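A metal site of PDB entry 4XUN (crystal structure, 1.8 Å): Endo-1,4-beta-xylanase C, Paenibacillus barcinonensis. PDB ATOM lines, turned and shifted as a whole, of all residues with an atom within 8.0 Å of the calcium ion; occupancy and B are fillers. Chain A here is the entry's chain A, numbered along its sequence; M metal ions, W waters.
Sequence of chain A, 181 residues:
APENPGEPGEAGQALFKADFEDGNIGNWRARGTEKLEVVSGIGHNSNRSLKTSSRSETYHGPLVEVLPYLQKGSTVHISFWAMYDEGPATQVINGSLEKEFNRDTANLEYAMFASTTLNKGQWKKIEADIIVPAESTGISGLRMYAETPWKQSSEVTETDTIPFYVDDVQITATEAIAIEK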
ATOM      1  N   ALA A  18      -7.990 -16.260  16.266  1.00  0.00           N
ATOM      2  CA  ALA A  18      -8.482 -15.442  15.171  1.00  0.00           C
ATOM      3  C   ALA A  18     -10.029 -15.476  15.183  1.00  0.00           C
ATOM      4  O   ALA A  18     -10.655 -16.541  14.984  1.00  0.00           O
ATOM      5  CB  ALA A  18      -7.961 -15.943  13.859  1.00  0.00           C
ATOM      6  N   ASP A  19     -10.624 -14.335  15.458  1.00  0.00           N
ATOM      7  CA  ASP A  19     -12.091 -14.208  15.454  1.00  0.00           C
ATOM      8  C   ASP A  19     -12.618 -13.301  14.334  1.00  0.00           C
ATOM      9  O   ASP A  19     -13.832 -13.210  14.139  1.00  0.00           O
ATOM     10  CB  ASP A  19     -12.616 -13.718  16.816  1.00  0.00           C
ATOM     11  CG  ASP A  19     -12.119 -12.327  17.220  1.00  0.00           C
ATOM     12  OD1 ASP A  19     -11.750 -11.493  16.364  1.00  0.00           O
ATOM     13  OD2 ASP A  19     -12.101 -12.087  18.456  1.00  0.00           O
ATOM     14  N   PHE A  20     -11.690 -12.662  13.615  1.00  0.00           N
ATOM     15  CA  PHE A  20     -11.955 -11.836  12.446  1.00  0.00           C
ATOM     16  C   PHE A  20     -12.762 -10.577  12.688  1.00  0.00           C
ATOM     17  O   PHE A  20     -13.199  -9.918  11.766  1.00  0.00           O
ATOM     18  CB  PHE A  20     -12.524 -12.700  11.315  1.00  0.00           C
ATOM     19  CG  PHE A  20     -11.668 -13.876  10.987  1.00  0.00           C
ATOM     20  CD1 PHE A  20     -10.495 -13.687  10.276  1.00  0.00           C
ATOM     21  CD2 PHE A  20     -11.989 -15.134  11.451  1.00  0.00           C
ATOM     22  CE1 PHE A  20      -9.674 -14.762   9.995  1.00  0.00           C
ATOM     23  CE2 PHE A  20     -11.162 -16.213  11.177  1.00  0.00           C
ATOM     24  CZ  PHE A  20     -10.003 -16.023  10.463  1.00  0.00           C
ATOM     25  N   GLU A  21     -12.973 -10.248  13.954  1.00  0.00           N
ATOM     26  CA  GLU A  21     -13.924  -9.176  14.296  1.00  0.00           C
ATOM     27  C   GLU A  21     -13.353  -7.792  13.956  1.00  0.00           C
ATOM     28  O   GLU A  21     -14.101  -6.832  13.820  1.00  0.00           O
ATOM     29  CB  GLU A  21     -14.340  -9.277  15.782  1.00  0.00           C
ATOM     30  CG  GLU A  21     -15.160 -10.512  16.142  1.00  0.00           C
ATOM     31  CD  GLU A  21     -16.388 -10.652  15.260  1.00  0.00           C
ATOM     32  OE1 GLU A  21     -17.167  -9.656  15.189  1.00  0.00           O
ATOM     33  OE2 GLU A  21     -16.596 -11.724  14.655  1.00  0.00           O
ATOM     34  N   ASP A  22     -12.031  -7.696  13.841  1.00  0.00           N
ATOM     35  CA  ASP A  22     -11.380  -6.481  13.340  1.00  0.00           C
ATOM     36  C   ASP A  22     -11.472  -6.310  11.818  1.00  0.00           C
ATOM     37  O   ASP A  22     -11.021  -5.299  11.290  1.00  0.00           O
ATOM     38  CB  ASP A  22      -9.924  -6.415  13.783  1.00  0.00           C
ATOM     39  CG  ASP A  22      -9.080  -7.632  13.353  1.00  0.00           C
ATOM     40  OD1 ASP A  22      -9.542  -8.506  12.573  1.00  0.00           O
ATOM     41  OD2 ASP A  22      -7.924  -7.715  13.865  1.00  0.00           O
ATOM     42  N   VAL A  38     -12.577 -11.748   4.448  1.00  0.00           N
ATOM     43  CA  VAL A  38     -13.277 -11.603   5.725  1.00  0.00           C
ATOM     44  C   VAL A  38     -14.615 -10.936   5.435  1.00  0.00           C
ATOM     45  O   VAL A  38     -14.640  -9.843   4.868  1.00  0.00           O
ATOM     46  CB  VAL A  38     -12.498 -10.783   6.731  1.00  0.00           C
ATOM     47  CG1 VAL A  38     -13.288 -10.613   8.004  1.00  0.00           C
ATOM     48  CG2 VAL A  38     -11.137 -11.450   7.019  1.00  0.00           C
ATOM     49  N   VAL A  39     -15.691 -11.622   5.790  1.00  0.00           N
ATOM     50  CA  VAL A  39     -17.026 -11.147   5.484  1.00  0.00           C
ATOM     51  C   VAL A  39     -17.692 -10.617   6.740  1.00  0.00           C
ATOM     52  O   VAL A  39     -17.265 -10.927   7.837  1.00  0.00           O
ATOM     53  CB  VAL A  39     -17.914 -12.263   4.905  1.00  0.00           C
ATOM     54  CG1 VAL A  39     -17.348 -12.772   3.585  1.00  0.00           C
ATOM     55  CG2 VAL A  39     -18.123 -13.392   5.915  1.00  0.00           C
ATOM     56  N   ILE A  42     -21.907 -12.555   8.810  1.00  0.00           N
ATOM     57  CA  ILE A  42     -21.852 -14.016   8.958  1.00  0.00           C
ATOM     58  C   ILE A  42     -20.702 -14.295   9.914  1.00  0.00           C
ATOM     59  O   ILE A  42     -19.567 -13.873   9.653  1.00  0.00           O
ATOM     60  CB  ILE A  42     -21.540 -14.751   7.612  1.00  0.00           C
ATOM     61  CG1 ILE A  42     -22.635 -14.511   6.548  1.00  0.00           C
ATOM     62  CG2 ILE A  42     -21.381 -16.254   7.800  1.00  0.00           C
ATOM     63  CD1 ILE A  42     -23.901 -15.294   6.856  1.00  0.00           C
ATOM     64  N   GLY A  43     -21.008 -14.967  11.013  1.00  0.00           N
ATOM     65  CA  GLY A  43     -19.973 -15.382  11.957  1.00  0.00           C
ATOM     66  C   GLY A  43     -20.526 -16.341  12.970  1.00  0.00           C
ATOM     67  O   GLY A  43     -21.748 -16.542  13.070  1.00  0.00           O
ATOM     68  N   HIS A  44     -19.634 -16.987  13.705  1.00  0.00           N
ATOM     69  CA  HIS A  44     -20.031 -17.822  14.801  1.00  0.00           C
ATOM     70  C   HIS A  44     -20.279 -16.963  16.045  1.00  0.00           C
ATOM     71  O   HIS A  44     -19.352 -16.389  16.624  1.00  0.00           O
ATOM     72  CB  HIS A  44     -18.954 -18.887  15.079  1.00  0.00           C
ATOM     73  CG  HIS A  44     -19.237 -19.723  16.292  1.00  0.00           C
ATOM     74  ND1 HIS A  44     -20.366 -20.506  16.428  1.00  0.00           N
ATOM     75  CD2 HIS A  44     -18.524 -19.877  17.423  1.00  0.00           C
ATOM     76  CE1 HIS A  44     -20.339 -21.110  17.605  1.00  0.00           C
ATOM     77  NE2 HIS A  44     -19.234 -20.745  18.222  1.00  0.00           N
ATOM     78  N   ASN A  45     -21.547 -16.827  16.417  1.00  0.00           N
ATOM     79  CA  ASN A  45     -21.922 -15.965  17.541  1.00  0.00           C
ATOM     80  C   ASN A  45     -21.174 -14.648  17.504  1.00  0.00           C
ATOM     81  O   ASN A  45     -20.620 -14.201  18.512  1.00  0.00           O
ATOM     82  CB  ASN A  45     -21.675 -16.668  18.898  1.00  0.00           C
ATOM     83  CG  ASN A  45     -22.443 -17.999  19.060  1.00  0.00           C
ATOM     84  OD1 ASN A  45     -22.022 -18.849  19.850  1.00  0.00           O
ATOM     85  ND2 ASN A  45     -23.535 -18.192  18.333  1.00  0.00           N
ATOM     86  N   SER A  46     -21.126 -14.058  16.309  1.00  0.00           N
ATOM     87  CA  SER A  46     -20.338 -12.902  16.024  1.00  0.00           C
ATOM     88  C   SER A  46     -20.657 -12.415  14.612  1.00  0.00           C
ATOM     89  O   SER A  46     -21.350 -13.136  13.842  1.00  0.00           O
ATOM     90  CB  SER A  46     -18.846 -13.221  16.154  1.00  0.00           C
ATOM     91  OG  SER A  46     -18.458 -14.167  15.162  1.00  0.00           O
ATOM     92  N   ASN A  47     -20.176 -11.220  14.257  1.00  0.00           N
ATOM     93  CA  ASN A  47     -20.522 -10.597  12.981  1.00  0.00           C
ATOM     94  C   ASN A  47     -19.564 -10.882  11.851  1.00  0.00           C
ATOM     95  O   ASN A  47     -19.861 -10.559  10.698  1.00  0.00           O
ATOM     96  CB  ASN A  47     -20.644  -9.060  13.123  1.00  0.00           C
ATOM     97  CG  ASN A  47     -21.459  -8.415  11.983  1.00  0.00           C
ATOM     98  OD1 ASN A  47     -22.557  -8.871  11.630  1.00  0.00           O
ATOM     99  ND2 ASN A  47     -20.919  -7.360  11.403  1.00  0.00           N
ATOM    100  N   ARG A  48     -18.380 -11.428  12.149  1.00  0.00           N
ATOM    101  CA  ARG A  48     -17.407 -11.615  11.068  1.00  0.00           C
ATOM    102  C   ARG A  48     -16.756 -12.999  11.055  1.00  0.00           C
ATOM    103  O   ARG A  48     -16.606 -13.608  12.094  1.00  0.00           O
ATOM    104  CB  ARG A  48     -16.347 -10.500  11.099  1.00  0.00           C
ATOM    105  CG  ARG A  48     -16.949  -9.099  10.957  1.00  0.00           C
ATOM    106  CD  ARG A  48     -15.980  -8.089  10.387  1.00  0.00           C
ATOM    107  NE  ARG A  48     -16.555  -6.740  10.475  1.00  0.00           N
ATOM    108  CZ  ARG A  48     -16.102  -5.657   9.837  1.00  0.00           C
ATOM    109  NH1 ARG A  48     -15.113  -5.710   8.967  1.00  0.00           N
ATOM    110  NH2 ARG A  48     -16.720  -4.492  10.062  1.00  0.00           N
ATOM    111  N   SER A  49     -16.353 -13.421   9.861  1.00  0.00           N
ATOM    112  CA  SER A  49     -15.685 -14.719   9.708  1.00  0.00           C
ATOM    113  C   SER A  49     -14.934 -14.746   8.388  1.00  0.00           C
ATOM    114  O   SER A  49     -14.960 -13.761   7.627  1.00  0.00           O
ATOM    115  CB  SER A  49     -16.681 -15.841   9.787  1.00  0.00           C
ATOM    116  OG  SER A  49     -17.615 -15.762   8.731  1.00  0.00           O
ATOM    117  N   LEU A  50     -14.188 -15.831   8.154  1.00  0.00           N
ATOM    118  CA  LEU A  50     -13.318 -15.932   6.989  1.00  0.00           C
ATOM    119  C   LEU A  50     -13.923 -16.877   5.987  1.00  0.00           C
ATOM    120  O   LEU A  50     -14.115 -18.059   6.256  1.00  0.00           O
ATOM    121  CB  LEU A  50     -11.950 -16.427   7.406  1.00  0.00           C
ATOM    122  CG  LEU A  50     -10.979 -16.659   6.280  1.00  0.00           C
ATOM    123  CD1 LEU A  50     -10.661 -15.368   5.535  1.00  0.00           C
ATOM    124  CD2 LEU A  50      -9.713 -17.274   6.840  1.00  0.00           C
ATOM    125  N   TRP A 123     -23.143 -23.942  12.331  1.00  0.00           N
ATOM    126  CA  TRP A 123     -21.740 -23.898  12.774  1.00  0.00           C
ATOM    127  C   TRP A 123     -21.423 -25.149  13.600  1.00  0.00           C
ATOM    128  O   TRP A 123     -22.232 -25.559  14.464  1.00  0.00           O
ATOM    129  CB  TRP A 123     -21.473 -22.619  13.594  1.00  0.00           C
ATOM    130  CG  TRP A 123     -21.501 -21.367  12.780  1.00  0.00           C
ATOM    131  CD1 TRP A 123     -22.580 -20.559  12.511  1.00  0.00           C
ATOM    132  CD2 TRP A 123     -20.390 -20.797  12.085  1.00  0.00           C
ATOM    133  NE1 TRP A 123     -22.204 -19.523  11.695  1.00  0.00           N
ATOM    134  CE2 TRP A 123     -20.849 -19.631  11.447  1.00  0.00           C
ATOM    135  CE3 TRP A 123     -19.040 -21.135  11.977  1.00  0.00           C
ATOM    136  CZ2 TRP A 123     -20.015 -18.832  10.673  1.00  0.00           C
ATOM    137  CZ3 TRP A 123     -18.191 -20.329  11.210  1.00  0.00           C
ATOM    138  CH2 TRP A 123     -18.686 -19.198  10.579  1.00  0.00           C
ATOM    139  N   VAL A 166     -14.842 -20.193   8.114  1.00  0.00           N
ATOM    140  CA  VAL A 166     -14.241 -20.547   9.396  1.00  0.00           C
ATOM    141  C   VAL A 166     -14.248 -19.335  10.346  1.00  0.00           C
ATOM    142  O   VAL A 166     -14.203 -18.173   9.934  1.00  0.00           O
ATOM    143  CB  VAL A 166     -12.810 -21.147   9.277  1.00  0.00           C
ATOM    144  CG1 VAL A 166     -12.827 -22.372   8.403  1.00  0.00           C
ATOM    145  CG2 VAL A 166     -11.797 -20.124   8.749  1.00  0.00           C
ATOM    146  N   ASP A 167     -14.273 -19.625  11.631  1.00  0.00           N
ATOM    147  CA  ASP A 167     -14.315 -18.597  12.647  1.00  0.00           C
ATOM    148  C   ASP A 167     -13.780 -19.157  13.993  1.00  0.00           C
ATOM    149  O   ASP A 167     -13.645 -20.348  14.151  1.00  0.00           O
ATOM    150  CB  ASP A 167     -15.740 -18.099  12.817  1.00  0.00           C
ATOM    151  CG  ASP A 167     -15.806 -16.705  13.451  1.00  0.00           C
ATOM    152  OD1 ASP A 167     -14.760 -16.043  13.718  1.00  0.00           O
ATOM    153  OD2 ASP A 167     -16.934 -16.235  13.717  1.00  0.00           O
ATOM    154  N   ASP A 168     -13.438 -18.263  14.903  1.00  0.00           N
ATOM    155  CA  ASP A 168     -13.045 -18.604  16.281  1.00  0.00           C
ATOM    156  C   ASP A 168     -11.983 -19.681  16.277  1.00  0.00           C
ATOM    157  O   ASP A 168     -12.111 -20.702  16.957  1.00  0.00           O
ATOM    158  CB  ASP A 168     -14.285 -19.014  17.089  1.00  0.00           C
ATOM    159  CG  ASP A 168     -15.151 -17.834  17.503  1.00  0.00           C
ATOM    160  OD1 ASP A 168     -14.654 -16.691  17.424  1.00  0.00           O
ATOM    161  OD2 ASP A 168     -16.336 -18.068  17.862  1.00  0.00           O
ATOM    162  N   VAL A 169     -10.910 -19.416  15.527  1.00  0.00           N
ATOM    163  CA  VAL A 169      -9.783 -20.315  15.447  1.00  0.00           C
ATOM    164  C   VAL A 169      -8.952 -20.062  16.693  1.00  0.00           C
ATOM    165  O   VAL A 169      -8.631 -18.895  17.020  1.00  0.00           O
ATOM    166  CB  VAL A 169      -8.933 -20.056  14.196  1.00  0.00           C
ATOM    167  CG1 VAL A 169      -7.770 -21.035  14.144  1.00  0.00           C
ATOM    168  CG2 VAL A 169      -9.772 -20.141  12.944  1.00  0.00           C
HETATM  169 CA    CA M   1     -16.029 -14.008  14.373  1.00  0.00          CA
HETATM  170  O   HOH W   1     -15.797 -14.457  16.604  1.00  0.00           O
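The side-chain carboxylate (OD2) of Asp 167 sits close to the backbone NH (N) of His 44, at 2.8 Å. The backbone carbonyl oxygen (O) of His 44 lies close to the side-chain hydroxyl (OG) of Ser 46.
The nearest printed residue that does not touch the calcium ion is Asp 168 (4.3 Å).
The calcium ion is bound by water W1, at 2.3 Å. The calcium ion is bound by O of Asp 19. The calcium ion is bound by the side-chain carboxylate (OE2) of Glu 21 (2.4 Å). O of Arg 48 binds the calcium ion (2.4 Å). The calcium ion is bound by the side-chain carboxylate (OD1) of Asp 167 (2.5 Å). OD2 of Asp 167 is bound to the calcium ion, 2.5 Å away. The calcium ion is bound by the side-chain hydroxyl (OG) of Ser 46, 2.6 Å away.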
